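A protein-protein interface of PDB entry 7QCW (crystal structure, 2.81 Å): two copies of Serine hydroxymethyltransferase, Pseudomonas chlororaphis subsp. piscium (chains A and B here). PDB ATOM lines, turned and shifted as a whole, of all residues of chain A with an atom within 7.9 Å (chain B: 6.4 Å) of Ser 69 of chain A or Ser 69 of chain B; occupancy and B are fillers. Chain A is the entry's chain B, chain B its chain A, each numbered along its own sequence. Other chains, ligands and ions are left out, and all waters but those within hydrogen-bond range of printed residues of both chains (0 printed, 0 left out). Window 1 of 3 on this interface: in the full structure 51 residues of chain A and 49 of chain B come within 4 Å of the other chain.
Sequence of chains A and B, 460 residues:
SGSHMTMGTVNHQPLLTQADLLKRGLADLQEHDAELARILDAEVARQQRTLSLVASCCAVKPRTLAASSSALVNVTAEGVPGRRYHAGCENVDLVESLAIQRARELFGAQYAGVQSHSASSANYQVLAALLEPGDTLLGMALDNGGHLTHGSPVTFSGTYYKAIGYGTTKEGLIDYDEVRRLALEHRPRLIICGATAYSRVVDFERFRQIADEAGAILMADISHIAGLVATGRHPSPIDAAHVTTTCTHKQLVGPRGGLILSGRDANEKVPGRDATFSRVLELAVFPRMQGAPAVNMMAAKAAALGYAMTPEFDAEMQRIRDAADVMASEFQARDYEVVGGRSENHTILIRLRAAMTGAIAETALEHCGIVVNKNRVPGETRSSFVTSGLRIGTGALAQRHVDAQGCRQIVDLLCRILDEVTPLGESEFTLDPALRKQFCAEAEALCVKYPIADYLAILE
Leu 65 of chain B touches Leu 21 of chain A. Ala 66 of chain B touches Leu 26 of chain A (CB to N, 3.7 Å). Leu 65 of chain A touches Leu 22 of chain B (CB to CD2, 3.9 Å). Leu 65 of chain A touches Val 73 of chain B (CD2 to CG1, 3.6 Å). Ser 68 of chain A touches Ser 68 of chain B (O to OG, 3.9 Å). Ser 68 of chain B touches Ser 69 of chain A. Leu 40 of chain B touches Ser 70 of chain A.
Hydrophobic or aromatic side chains of chain A within 4 Å of the printed part of chain B: Leu 21, Leu 26, Leu 29, Leu 40, Val 60, Pro 62, Leu 65 and Tyr 455. Of the 15 printed residues of chain B, 11 touch a printed residue of chain A. Hydrophobic or aromatic side chains of chain B that line the printed part of chain A: Leu 21, Leu 22, Leu 40, Leu 65, Ala 66, Ala 67, Ala 71 and Val 73. Among the printed residues, 23 pairs touch across the chains.
O of Leu 40 of chain B lies close to OE1 of Gln 18 of chain A (3.5 Å). The side-chain hydroxyl (OG) of Ser 69 of chain B lies within hydrogen-bond range of the backbone carbonyl oxygen (O) of Leu 65 of chain A. The backbone carbonyl oxygen (O) of Leu 65 of chain B is in hydrogen-bond range of the side-chain hydroxyl (OG) of Ser 69 of chain A (2.7 Å).
Leu 65 of chain A touches Leu 22 of chain B, but with the chains exchanged Leu 22 of chain A does not touch Leu 65 of chain B (4.5 Å). Ala 66 of chain A touches Leu 22 of chain B, but with the chains exchanged Leu 22 of chain A does not touch Ala 66 of chain B (4.9 Å). Positions printed for both chains: 21, 22, 40, 64, 65, 66, 67, 68, 69, 70, 71, 72, 73, 296 and 297.
The side-chain hydroxyl of Ser 70 of chain A is in hydrogen-bond range of the backbone NH of Leu 72 of chain A (2.8 Å). The backbone carbonyl oxygen (O) of Leu 65 of chain B sits at hydrogen-bond distance from the side-chain hydroxyl (OG) of Ser 68 of chain B (2.7 Å). The backbone carbonyl oxygen (O) of Ser 69 of chain A sits at hydrogen-bond distance from the side-chain amide nitrogen (NE2) of Gln 18 of chain A.
Of the printed residues of chain B, Val 60 of chain A touches Val 73. Of the printed residues of chain B, Ser 69 of chain A touches Leu 65 (2.7 Å), Ser 68 (3.8 Å) and Ser 69 (3.1 Å). Of the printed residues of chain A, Ala 66 of chain B touches Leu 26 and Leu 29. Of chain A, only Ser 68 (3.9 Å) and Ser 69 (3.8 Å) come within 4 Å of Ser 68 of chain B. Of chain A, only Leu 65 (2.4 Å), Ala 66 (3.9 Å) and Ser 69 (3.1 Å) come within 4 Å of Ser 69 of chain B. Leu 72 of chain B touches none of the printed residues of chain A. Asn 296 of chain B touches none of the printed residues of chain A. The nearest residue of chain B that does not touch Ser 69 of chain A is Ala 66 of chain B (4.5 Å). The nearest residue of chain A that does not touch Ser 69 of chain B is Ser 68 of chain A (4.4 Å).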
ATOM      1  N   GLN A  18      -9.038  20.083 -28.857  1.00  0.00           N
ATOM      2  CA  GLN A  18      -9.712  20.803 -27.781  1.00  0.00           C
ATOM      3  C   GLN A  18     -10.949  20.053 -27.308  1.00  0.00           C
ATOM      4  O   GLN A  18     -11.247  20.022 -26.109  1.00  0.00           O
ATOM      5  CB  GLN A  18     -10.085  22.209 -28.253  1.00  0.00           C
ATOM      6  CG  GLN A  18     -10.302  23.202 -27.130  1.00  0.00           C
ATOM      7  CD  GLN A  18      -9.116  23.277 -26.190  1.00  0.00           C
ATOM      8  OE1 GLN A  18      -8.097  23.886 -26.504  1.00  0.00           O
ATOM      9  NE2 GLN A  18      -9.236  22.645 -25.039  1.00  0.00           N
ATOM     10  N   ALA A  19     -11.689  19.449 -28.241  1.00  0.00           N
ATOM     11  CA  ALA A  19     -12.891  18.709 -27.872  1.00  0.00           C
ATOM     12  C   ALA A  19     -12.558  17.514 -26.986  1.00  0.00           C
ATOM     13  O   ALA A  19     -13.170  17.322 -25.927  1.00  0.00           O
ATOM     14  CB  ALA A  19     -13.634  18.261 -29.131  1.00  0.00           C
ATOM     15  N   LEU A  21      -9.855  16.843 -25.178  1.00  0.00           N
ATOM     16  CA  LEU A  21      -9.394  17.322 -23.878  1.00  0.00           C
ATOM     17  C   LEU A  21     -10.576  17.659 -22.977  1.00  0.00           C
ATOM     18  O   LEU A  21     -10.602  17.304 -21.793  1.00  0.00           O
ATOM     19  CB  LEU A  21      -8.499  18.547 -24.075  1.00  0.00           C
ATOM     20  CG  LEU A  21      -7.990  19.249 -22.818  1.00  0.00           C
ATOM     21  CD1 LEU A  21      -7.005  18.360 -22.087  1.00  0.00           C
ATOM     22  CD2 LEU A  21      -7.366  20.593 -23.163  1.00  0.00           C
ATOM     23  N   LEU A  22     -11.570  18.339 -23.545  1.00  0.00           N
ATOM     24  CA  LEU A  22     -12.746  18.775 -22.800  1.00  0.00           C
ATOM     25  C   LEU A  22     -13.724  17.638 -22.529  1.00  0.00           C
ATOM     26  O   LEU A  22     -14.309  17.577 -21.441  1.00  0.00           O
ATOM     27  CB  LEU A  22     -13.402  19.916 -23.570  1.00  0.00           C
ATOM     28  CG  LEU A  22     -12.868  21.291 -23.200  1.00  0.00           C
ATOM     29  CD1 LEU A  22     -11.394  21.436 -23.369  1.00  0.00           C
ATOM     30  CD2 LEU A  22     -13.539  22.205 -24.210  1.00  0.00           C
ATOM     31  N   LEU A  26     -14.850  16.832 -18.972  1.00  0.00           N
ATOM     32  CA  LEU A  26     -16.223  16.666 -18.505  1.00  0.00           C
ATOM     33  C   LEU A  26     -16.424  15.293 -17.877  1.00  0.00           C
ATOM     34  O   LEU A  26     -17.094  15.164 -16.845  1.00  0.00           O
ATOM     35  CB  LEU A  26     -17.200  16.877 -19.661  1.00  0.00           C
ATOM     36  CG  LEU A  26     -17.300  18.305 -20.200  1.00  0.00           C
ATOM     37  CD1 LEU A  26     -17.928  18.314 -21.585  1.00  0.00           C
ATOM     38  CD2 LEU A  26     -18.082  19.191 -19.244  1.00  0.00           C
ATOM     39  N   LEU A  29     -14.644  15.302 -14.534  1.00  0.00           N
ATOM     40  CA  LEU A  29     -15.497  15.948 -13.550  1.00  0.00           C
ATOM     41  C   LEU A  29     -16.881  15.295 -13.508  1.00  0.00           C
ATOM     42  O   LEU A  29     -17.911  15.979 -13.354  1.00  0.00           O
ATOM     43  CB  LEU A  29     -15.571  17.444 -13.880  1.00  0.00           C
ATOM     44  CG  LEU A  29     -16.400  18.427 -13.048  1.00  0.00           C
ATOM     45  CD1 LEU A  29     -15.670  18.677 -11.747  1.00  0.00           C
ATOM     46  CD2 LEU A  29     -16.673  19.728 -13.798  1.00  0.00           C
ATOM     47  N   LEU A  40     -23.323  22.066 -10.614  1.00  0.00           N
ATOM     48  CA  LEU A  40     -23.304  22.747 -11.905  1.00  0.00           C
ATOM     49  C   LEU A  40     -24.432  22.259 -12.806  1.00  0.00           C
ATOM     50  O   LEU A  40     -25.023  23.050 -13.552  1.00  0.00           O
ATOM     51  CB  LEU A  40     -21.945  22.553 -12.577  1.00  0.00           C
ATOM     52  CG  LEU A  40     -20.769  23.204 -11.846  1.00  0.00           C
ATOM     53  CD1 LEU A  40     -19.465  22.949 -12.582  1.00  0.00           C
ATOM     54  CD2 LEU A  40     -21.008  24.697 -11.668  1.00  0.00           C
ATOM     55  N   VAL A  60     -25.209  32.347 -22.153  1.00  0.00           N
ATOM     56  CA  VAL A  60     -24.144  32.295 -23.148  1.00  0.00           C
ATOM     57  C   VAL A  60     -24.341  31.098 -24.066  1.00  0.00           C
ATOM     58  O   VAL A  60     -24.757  30.015 -23.635  1.00  0.00           O
ATOM     59  CB  VAL A  60     -22.768  32.250 -22.462  1.00  0.00           C
ATOM     60  CG1 VAL A  60     -21.654  32.418 -23.487  1.00  0.00           C
ATOM     61  CG2 VAL A  60     -22.674  33.328 -21.397  1.00  0.00           C
ATOM     62  N   LYS A  61     -24.055  31.299 -25.350  1.00  0.00           N
ATOM     63  CA  LYS A  61     -24.224  30.233 -26.324  1.00  0.00           C
ATOM     64  C   LYS A  61     -23.227  29.109 -26.054  1.00  0.00           C
ATOM     65  O   LYS A  61     -22.090  29.370 -25.644  1.00  0.00           O
ATOM     66  CB  LYS A  61     -24.043  30.773 -27.739  1.00  0.00           C
ATOM     67  CG  LYS A  61     -25.044  31.854 -28.097  1.00  0.00           C
ATOM     68  CD  LYS A  61     -26.463  31.463 -27.685  1.00  0.00           C
ATOM     69  CE  LYS A  61     -27.507  32.255 -28.461  1.00  0.00           C
ATOM     70  NZ  LYS A  61     -28.893  32.069 -27.953  1.00  0.00           N
ATOM     71  N   PRO A  62     -23.625  27.851 -26.262  1.00  0.00           N
ATOM     72  CA  PRO A  62     -22.701  26.735 -25.991  1.00  0.00           C
ATOM     73  C   PRO A  62     -21.424  26.803 -26.807  1.00  0.00           C
ATOM     74  O   PRO A  62     -20.354  26.416 -26.320  1.00  0.00           O
ATOM     75  CB  PRO A  62     -23.543  25.499 -26.343  1.00  0.00           C
ATOM     76  CG  PRO A  62     -24.596  26.013 -27.281  1.00  0.00           C
ATOM     77  CD  PRO A  62     -24.921  27.382 -26.779  1.00  0.00           C
ATOM     78  N   ARG A  63     -21.515  27.288 -28.047  1.00  0.00           N
ATOM     79  CA  ARG A  63     -20.337  27.434 -28.895  1.00  0.00           C
ATOM     80  C   ARG A  63     -19.323  28.381 -28.263  1.00  0.00           C
ATOM     81  O   ARG A  63     -18.120  28.100 -28.243  1.00  0.00           O
ATOM     82  CB  ARG A  63     -20.779  27.918 -30.276  1.00  0.00           C
ATOM     83  CG  ARG A  63     -19.807  28.776 -31.062  1.00  0.00           C
ATOM     84  CD  ARG A  63     -20.475  29.132 -32.384  1.00  0.00           C
ATOM     85  NE  ARG A  63     -19.757  30.121 -33.179  1.00  0.00           N
ATOM     86  CZ  ARG A  63     -20.194  30.582 -34.347  1.00  0.00           C
ATOM     87  NH1 ARG A  63     -21.345  30.142 -34.842  1.00  0.00           N
ATOM     88  NH2 ARG A  63     -19.491  31.483 -35.019  1.00  0.00           N
ATOM     89  N   THR A  64     -19.799  29.506 -27.728  1.00  0.00           N
ATOM     90  CA  THR A  64     -18.918  30.415 -27.004  1.00  0.00           C
ATOM     91  C   THR A  64     -18.426  29.795 -25.700  1.00  0.00           C
ATOM     92  O   THR A  64     -17.278  30.023 -25.298  1.00  0.00           O
ATOM     93  CB  THR A  64     -19.643  31.736 -26.739  1.00  0.00           C
ATOM     94  OG1 THR A  64     -19.889  32.402 -27.984  1.00  0.00           O
ATOM     95  CG2 THR A  64     -18.811  32.647 -25.851  1.00  0.00           C
ATOM     96  N   LEU A  65     -19.271  29.004 -25.034  1.00  0.00           N
ATOM     97  CA  LEU A  65     -18.871  28.373 -23.779  1.00  0.00           C
ATOM     98  C   LEU A  65     -17.740  27.372 -23.987  1.00  0.00           C
ATOM     99  O   LEU A  65     -16.794  27.326 -23.193  1.00  0.00           O
ATOM    100  CB  LEU A  65     -20.073  27.691 -23.128  1.00  0.00           C
ATOM    101  CG  LEU A  65     -20.969  28.586 -22.275  1.00  0.00           C
ATOM    102  CD1 LEU A  65     -22.121  27.785 -21.691  1.00  0.00           C
ATOM    103  CD2 LEU A  65     -20.159  29.251 -21.176  1.00  0.00           C
ATOM    104  N   ALA A  66     -17.826  26.555 -25.040  1.00  0.00           N
ATOM    105  CA  ALA A  66     -16.797  25.547 -25.279  1.00  0.00           C
ATOM    106  C   ALA A  66     -15.445  26.192 -25.558  1.00  0.00           C
ATOM    107  O   ALA A  66     -14.401  25.661 -25.162  1.00  0.00           O
ATOM    108  CB  ALA A  66     -17.209  24.636 -26.435  1.00  0.00           C
ATOM    109  N   ALA A  67     -15.446  27.336 -26.248  1.00  0.00           N
ATOM    110  CA  ALA A  67     -14.201  28.059 -26.488  1.00  0.00           C
ATOM    111  C   ALA A  67     -13.548  28.502 -25.184  1.00  0.00           C
ATOM    112  O   ALA A  67     -12.325  28.671 -25.131  1.00  0.00           O
ATOM    113  CB  ALA A  67     -14.461  29.265 -27.390  1.00  0.00           C
ATOM    114  N   SER A  68     -14.342  28.687 -24.126  1.00  0.00           N
ATOM    115  CA  SER A  68     -13.815  29.146 -22.846  1.00  0.00           C
ATOM    116  C   SER A  68     -13.003  28.084 -22.116  1.00  0.00           C
ATOM    117  O   SER A  68     -12.327  28.415 -21.137  1.00  0.00           O
ATOM    118  CB  SER A  68     -14.957  29.621 -21.946  1.00  0.00           C
ATOM    119  OG  SER A  68     -15.612  30.745 -22.504  1.00  0.00           O
ATOM    120  N   SER A  69     -13.056  26.827 -22.552  1.00  0.00           N
ATOM    121  CA  SER A  69     -12.216  25.784 -21.983  1.00  0.00           C
ATOM    122  C   SER A  69     -10.971  25.536 -22.823  1.00  0.00           C
ATOM    123  O   SER A  69     -10.426  24.427 -22.815  1.00  0.00           O
ATOM    124  CB  SER A  69     -13.014  24.496 -21.806  1.00  0.00           C
ATOM    125  OG  SER A  69     -14.126  24.689 -20.953  1.00  0.00           O
ATOM    126  N   SER A  70     -10.524  26.553 -23.553  1.00  0.00           N
ATOM    127  CA  SER A  70      -9.279  26.482 -24.298  1.00  0.00           C
ATOM    128  C   SER A  70      -8.105  26.173 -23.379  1.00  0.00           C
ATOM    129  O   SER A  70      -8.089  26.554 -22.206  1.00  0.00           O
ATOM    130  CB  SER A  70      -9.021  27.808 -25.002  1.00  0.00           C
ATOM    131  OG  SER A  70      -7.741  27.810 -25.602  1.00  0.00           O
ATOM    132  N   ALA A  71      -7.107  25.483 -23.930  1.00  0.00           N
ATOM    133  CA  ALA A  71      -5.829  25.320 -23.251  1.00  0.00           C
ATOM    134  C   ALA A  71      -4.937  26.543 -23.402  1.00  0.00           C
ATOM    135  O   ALA A  71      -3.827  26.559 -22.860  1.00  0.00           O
ATOM    136  CB  ALA A  71      -5.101  24.077 -23.773  1.00  0.00           C
ATOM    137  N   LEU A  72      -5.404  27.564 -24.122  1.00  0.00           N
ATOM    138  CA  LEU A  72      -4.722  28.851 -24.165  1.00  0.00           C
ATOM    139  C   LEU A  72      -4.683  29.516 -22.796  1.00  0.00           C
ATOM    140  O   LEU A  72      -3.921  30.471 -22.598  1.00  0.00           O
ATOM    141  CB  LEU A  72      -5.413  29.749 -25.189  1.00  0.00           C
ATOM    142  CG  LEU A  72      -5.070  29.478 -26.653  1.00  0.00           C
ATOM    143  CD1 LEU A  72      -6.012  30.200 -27.589  1.00  0.00           C
ATOM    144  CD2 LEU A  72      -3.665  29.945 -26.915  1.00  0.00           C
ATOM    145  N   VAL A  73      -5.502  29.038 -21.855  1.00  0.00           N
ATOM    146  CA  VAL A  73      -5.387  29.459 -20.461  1.00  0.00           C
ATOM    147  C   VAL A  73      -3.980  29.191 -19.938  1.00  0.00           C
ATOM    148  O   VAL A  73      -3.445  29.958 -19.128  1.00  0.00           O
ATOM    149  CB  VAL A  73      -6.461  28.755 -19.606  1.00  0.00           C
ATOM    150  CG1 VAL A  73      -6.306  27.240 -19.674  1.00  0.00           C
ATOM    151  CG2 VAL A  73      -6.395  29.226 -18.160  1.00  0.00           C
ATOM    152  N   ASN A  74      -3.349  28.111 -20.410  1.00  0.00           N
ATOM    153  CA  ASN A  74      -2.014  27.745 -19.954  1.00  0.00           C
ATOM    154  C   ASN A  74      -0.924  28.661 -20.497  1.00  0.00           C
ATOM    155  O   ASN A  74       0.231  28.536 -20.075  1.00  0.00           O
ATOM    156  CB  ASN A  74      -1.705  26.296 -20.336  1.00  0.00           C
ATOM    157  CG  ASN A  74      -2.847  25.352 -20.014  1.00  0.00           C
ATOM    158  OD1 ASN A  74      -3.523  25.506 -18.997  1.00  0.00           O
ATOM    159  ND2 ASN A  74      -3.050  24.355 -20.866  1.00  0.00           N
ATOM    160  N   ASN A 296      -8.204  32.252 -22.848  1.00  0.00           N
ATOM    161  CA  ASN A 296      -9.398  31.425 -23.003  1.00  0.00           C
ATOM    162  C   ASN A 296     -10.643  32.288 -23.186  1.00  0.00           C
ATOM    163  O   ASN A 296     -11.495  31.979 -24.026  1.00  0.00           O
ATOM    164  CB  ASN A 296      -9.563  30.480 -21.810  1.00  0.00           C
ATOM    165  CG  ASN A 296      -9.574  31.208 -20.483  1.00  0.00           C
ATOM    166  OD1 ASN A 296      -8.890  32.216 -20.308  1.00  0.00           O
ATOM    167  ND2 ASN A 296     -10.348  30.692 -19.533  1.00  0.00           N
ATOM    168  N   MET A 297     -10.766  33.380 -22.417  1.00  0.00           N
ATOM    169  CA  MET A 297     -11.859  34.317 -22.665  1.00  0.00           C
ATOM    170  C   MET A 297     -11.740  34.934 -24.052  1.00  0.00           C
ATOM    171  O   MET A 297     -12.755  35.241 -24.685  1.00  0.00           O
ATOM    172  CB  MET A 297     -11.900  35.457 -21.638  1.00  0.00           C
ATOM    173  CG  MET A 297     -12.129  35.098 -20.171  1.00  0.00           C
ATOM    174  SD  MET A 297     -13.626  34.217 -19.697  1.00  0.00           S
ATOM    175  CE  MET A 297     -12.927  32.580 -19.460  1.00  0.00           C
ATOM    176  N   ALA A 299     -10.607  33.578 -26.847  1.00  0.00           N
ATOM    177  CA  ALA A 299     -11.177  32.671 -27.833  1.00  0.00           C
ATOM    178  C   ALA A 299     -12.695  32.752 -27.808  1.00  0.00           C
ATOM    179  O   ALA A 299     -13.340  32.756 -28.863  1.00  0.00           O
ATOM    180  CB  ALA A 299     -10.707  31.236 -27.591  1.00  0.00           C
ATOM    181  N   ALA A 300     -13.283  32.851 -26.613  1.00  0.00           N
ATOM    182  CA  ALA A 300     -14.739  32.890 -26.491  1.00  0.00           C
ATOM    183  C   ALA A 300     -15.318  34.179 -27.077  1.00  0.00           C
ATOM    184  O   ALA A 300     -16.403  34.170 -27.673  1.00  0.00           O
ATOM    185  CB  ALA A 300     -15.134  32.719 -25.022  1.00  0.00           C
ATOM    186  N   TYR A 455     -30.174  25.647 -25.626  1.00  0.00           N
ATOM    187  CA  TYR A 455     -29.822  24.777 -24.513  1.00  0.00           C
ATOM    188  C   TYR A 455     -30.516  23.422 -24.600  1.00  0.00           C
ATOM    189  O   TYR A 455     -30.489  22.660 -23.628  1.00  0.00           O
ATOM    190  CB  TYR A 455     -30.148  25.464 -23.184  1.00  0.00           C
ATOM    191  CG  TYR A 455     -28.998  26.279 -22.625  1.00  0.00           C
ATOM    192  CD1 TYR A 455     -28.229  27.088 -23.452  1.00  0.00           C
ATOM    193  CD2 TYR A 455     -28.679  26.234 -21.273  1.00  0.00           C
ATOM    194  CE1 TYR A 455     -27.176  27.832 -22.949  1.00  0.00           C
ATOM    195  CE2 TYR A 455     -27.627  26.975 -20.761  1.00  0.00           C
ATOM    196  CZ  TYR A 455     -26.879  27.772 -21.604  1.00  0.00           C
ATOM    197  OH  TYR A 455     -25.833  28.512 -21.101  1.00  0.00           O
ATOM    198  N   LEU B  21     -24.570  19.793 -22.925  1.00  0.00           N
ATOM    199  CA  LEU B  21     -24.531  21.200 -23.308  1.00  0.00           C
ATOM    200  C   LEU B  21     -23.172  21.580 -23.882  1.00  0.00           C
ATOM    201  O   LEU B  21     -23.085  22.189 -24.956  1.00  0.00           O
ATOM    202  CB  LEU B  21     -24.864  22.066 -22.090  1.00  0.00           C
ATOM    203  CG  LEU B  21     -24.825  23.588 -22.224  1.00  0.00           C
ATOM    204  CD1 LEU B  21     -26.040  24.100 -22.983  1.00  0.00           C
ATOM    205  CD2 LEU B  21     -24.731  24.236 -20.851  1.00  0.00           C
ATOM    206  N   LEU B  22     -22.095  21.223 -23.178  1.00  0.00           N
ATOM    207  CA  LEU B  22     -20.756  21.569 -23.635  1.00  0.00           C
ATOM    208  C   LEU B  22     -20.278  20.674 -24.775  1.00  0.00           C
ATOM    209  O   LEU B  22     -19.575  21.155 -25.669  1.00  0.00           O
ATOM    210  CB  LEU B  22     -19.776  21.516 -22.459  1.00  0.00           C
ATOM    211  CG  LEU B  22     -19.743  22.804 -21.627  1.00  0.00           C
ATOM    212  CD1 LEU B  22     -18.862  22.638 -20.400  1.00  0.00           C
ATOM    213  CD2 LEU B  22     -19.282  23.966 -22.485  1.00  0.00           C
ATOM    214  N   LEU B  40      -7.537  26.604 -31.834  1.00  0.00           N
ATOM    215  CA  LEU B  40      -7.702  25.957 -30.537  1.00  0.00           C
ATOM    216  C   LEU B  40      -7.032  24.590 -30.520  1.00  0.00           C
ATOM    217  O   LEU B  40      -6.399  24.213 -29.526  1.00  0.00           O
ATOM    218  CB  LEU B  40      -9.186  25.837 -30.186  1.00  0.00           C
ATOM    219  CG  LEU B  40      -9.815  27.088 -29.567  1.00  0.00           C
ATOM    220  CD1 LEU B  40      -9.083  27.384 -28.311  1.00  0.00           C
ATOM    221  CD2 LEU B  40      -9.795  28.306 -30.458  1.00  0.00           C
ATOM    222  N   THR B  64     -10.720  20.893 -14.210  1.00  0.00           N
ATOM    223  CA  THR B  64     -10.821  22.318 -13.923  1.00  0.00           C
ATOM    224  C   THR B  64     -11.218  23.106 -15.166  1.00  0.00           C
ATOM    225  O   THR B  64     -11.938  24.107 -15.065  1.00  0.00           O
ATOM    226  CB  THR B  64      -9.491  22.819 -13.358  1.00  0.00           C
ATOM    227  OG1 THR B  64      -9.136  22.031 -12.215  1.00  0.00           O
ATOM    228  CG2 THR B  64      -9.596  24.272 -12.939  1.00  0.00           C
ATOM    229  N   LEU B  65     -10.762  22.671 -16.344  1.00  0.00           N
ATOM    230  CA  LEU B  65     -11.195  23.303 -17.586  1.00  0.00           C
ATOM    231  C   LEU B  65     -12.672  23.051 -17.860  1.00  0.00           C
ATOM    232  O   LEU B  65     -13.341  23.897 -18.464  1.00  0.00           O
ATOM    233  CB  LEU B  65     -10.350  22.803 -18.757  1.00  0.00           C
ATOM    234  CG  LEU B  65      -9.187  23.696 -19.191  1.00  0.00           C
ATOM    235  CD1 LEU B  65      -8.257  23.924 -18.040  1.00  0.00           C
ATOM    236  CD2 LEU B  65      -8.436  23.078 -20.354  1.00  0.00           C
ATOM    237  N   ALA B  66     -13.194  21.896 -17.439  1.00  0.00           N
ATOM    238  CA  ALA B  66     -14.610  21.611 -17.638  1.00  0.00           C
ATOM    239  C   ALA B  66     -15.484  22.513 -16.776  1.00  0.00           C
ATOM    240  O   ALA B  66     -16.508  23.025 -17.243  1.00  0.00           O
ATOM    241  CB  ALA B  66     -14.896  20.140 -17.338  1.00  0.00           C
ATOM    242  N   ALA B  67     -15.097  22.719 -15.514  1.00  0.00           N
ATOM    243  CA  ALA B  67     -15.891  23.560 -14.622  1.00  0.00           C
ATOM    244  C   ALA B  67     -15.821  25.029 -15.013  1.00  0.00           C
ATOM    245  O   ALA B  67     -16.745  25.793 -14.712  1.00  0.00           O
ATOM    246  CB  ALA B  67     -15.431  23.373 -13.177  1.00  0.00           C
ATOM    247  N   SER B  68     -14.744  25.445 -15.683  1.00  0.00           N
ATOM    248  CA  SER B  68     -14.587  26.842 -16.068  1.00  0.00           C
ATOM    249  C   SER B  68     -15.574  27.277 -17.142  1.00  0.00           C
ATOM    250  O   SER B  68     -15.687  28.480 -17.402  1.00  0.00           O
ATOM    251  CB  SER B  68     -13.159  27.098 -16.554  1.00  0.00           C
ATOM    252  OG  SER B  68     -12.944  26.527 -17.832  1.00  0.00           O
ATOM    253  N   SER B  69     -16.283  26.341 -17.773  1.00  0.00           N
ATOM    254  CA  SER B  69     -17.251  26.660 -18.815  1.00  0.00           C
ATOM    255  C   SER B  69     -18.664  26.259 -18.407  1.00  0.00           C
ATOM    256  O   SER B  69     -19.480  25.888 -19.252  1.00  0.00           O
ATOM    257  CB  SER B  69     -16.868  25.993 -20.134  1.00  0.00           C
ATOM    258  OG  SER B  69     -17.760  26.379 -21.162  1.00  0.00           O
ATOM    259  N   SER B  70     -18.959  26.327 -17.112  1.00  0.00           N
ATOM    260  CA  SER B  70     -20.298  26.038 -16.631  1.00  0.00           C
ATOM    261  C   SER B  70     -21.290  27.071 -17.162  1.00  0.00           C
ATOM    262  O   SER B  70     -20.920  28.134 -17.669  1.00  0.00           O
ATOM    263  CB  SER B  70     -20.323  26.025 -15.103  1.00  0.00           C
ATOM    264  OG  SER B  70     -19.874  27.265 -14.581  1.00  0.00           O
ATOM    265  N   ALA B  71     -22.574  26.743 -17.042  1.00  0.00           N
ATOM    266  CA  ALA B  71     -23.629  27.703 -17.331  1.00  0.00           C
ATOM    267  C   ALA B  71     -23.818  28.705 -16.203  1.00  0.00           C
ATOM    268  O   ALA B  71     -24.688  29.577 -16.302  1.00  0.00           O
ATOM    269  CB  ALA B  71     -24.947  26.978 -17.612  1.00  0.00           C
ATOM    270  N   LEU B  72     -23.016  28.603 -15.142  1.00  0.00           N
ATOM    271  CA  LEU B  72     -23.027  29.552 -14.041  1.00  0.00           C
ATOM    272  C   LEU B  72     -22.477  30.911 -14.458  1.00  0.00           C
ATOM    273  O   LEU B  72     -22.445  31.837 -13.642  1.00  0.00           O
ATOM    274  CB  LEU B  72     -22.227  28.960 -12.877  1.00  0.00           C
ATOM    275  CG  LEU B  72     -22.316  29.549 -11.475  1.00  0.00           C
ATOM    276  CD1 LEU B  72     -23.742  29.431 -10.999  1.00  0.00           C
ATOM    277  CD2 LEU B  72     -21.398  28.774 -10.552  1.00  0.00           C
ATOM    278  N   VAL B  73     -22.029  31.035 -15.710  1.00  0.00           N
ATOM    279  CA  VAL B  73     -21.694  32.331 -16.291  1.00  0.00           C
ATOM    280  C   VAL B  73     -22.949  33.166 -16.516  1.00  0.00           C
ATOM    281  O   VAL B  73     -22.912  34.398 -16.411  1.00  0.00           O
ATOM    282  CB  VAL B  73     -20.908  32.123 -17.599  1.00  0.00           C
ATOM    283  CG1 VAL B  73     -21.690  31.233 -18.552  1.00  0.00           C
ATOM    284  CG2 VAL B  73     -20.583  33.457 -18.255  1.00  0.00           C
ATOM    285  N   ASN B 296     -17.770  31.438 -12.963  1.00  0.00           N
ATOM    286  CA  ASN B 296     -17.165  30.244 -13.538  1.00  0.00           C
ATOM    287  C   ASN B 296     -15.906  29.871 -12.773  1.00  0.00           C
ATOM    288  O   ASN B 296     -15.697  28.704 -12.417  1.00  0.00           O
ATOM    289  CB  ASN B 296     -16.784  30.558 -14.984  1.00  0.00           C
ATOM    290  CG  ASN B 296     -17.953  31.015 -15.795  1.00  0.00           C
ATOM    291  OD1 ASN B 296     -18.055  32.187 -16.176  1.00  0.00           O
ATOM    292  ND2 ASN B 296     -18.820  30.069 -16.139  1.00  0.00           N
ATOM    293  N   MET B 297     -15.051  30.876 -12.501  1.00  0.00           N
ATOM    294  CA  MET B 297     -13.765  30.619 -11.867  1.00  0.00           C
ATOM    295  C   MET B 297     -13.971  30.133 -10.447  1.00  0.00           C
ATOM    296  O   MET B 297     -13.085  29.494  -9.881  1.00  0.00           O
ATOM    297  CB  MET B 297     -12.877  31.862 -11.864  1.00  0.00           C
ATOM    298  CG  MET B 297     -12.632  32.497 -13.242  1.00  0.00           C
ATOM    299  SD  MET B 297     -12.054  31.501 -14.644  1.00  0.00           S
ATOM    300  CE  MET B 297     -13.605  31.307 -15.511  1.00  0.00           C
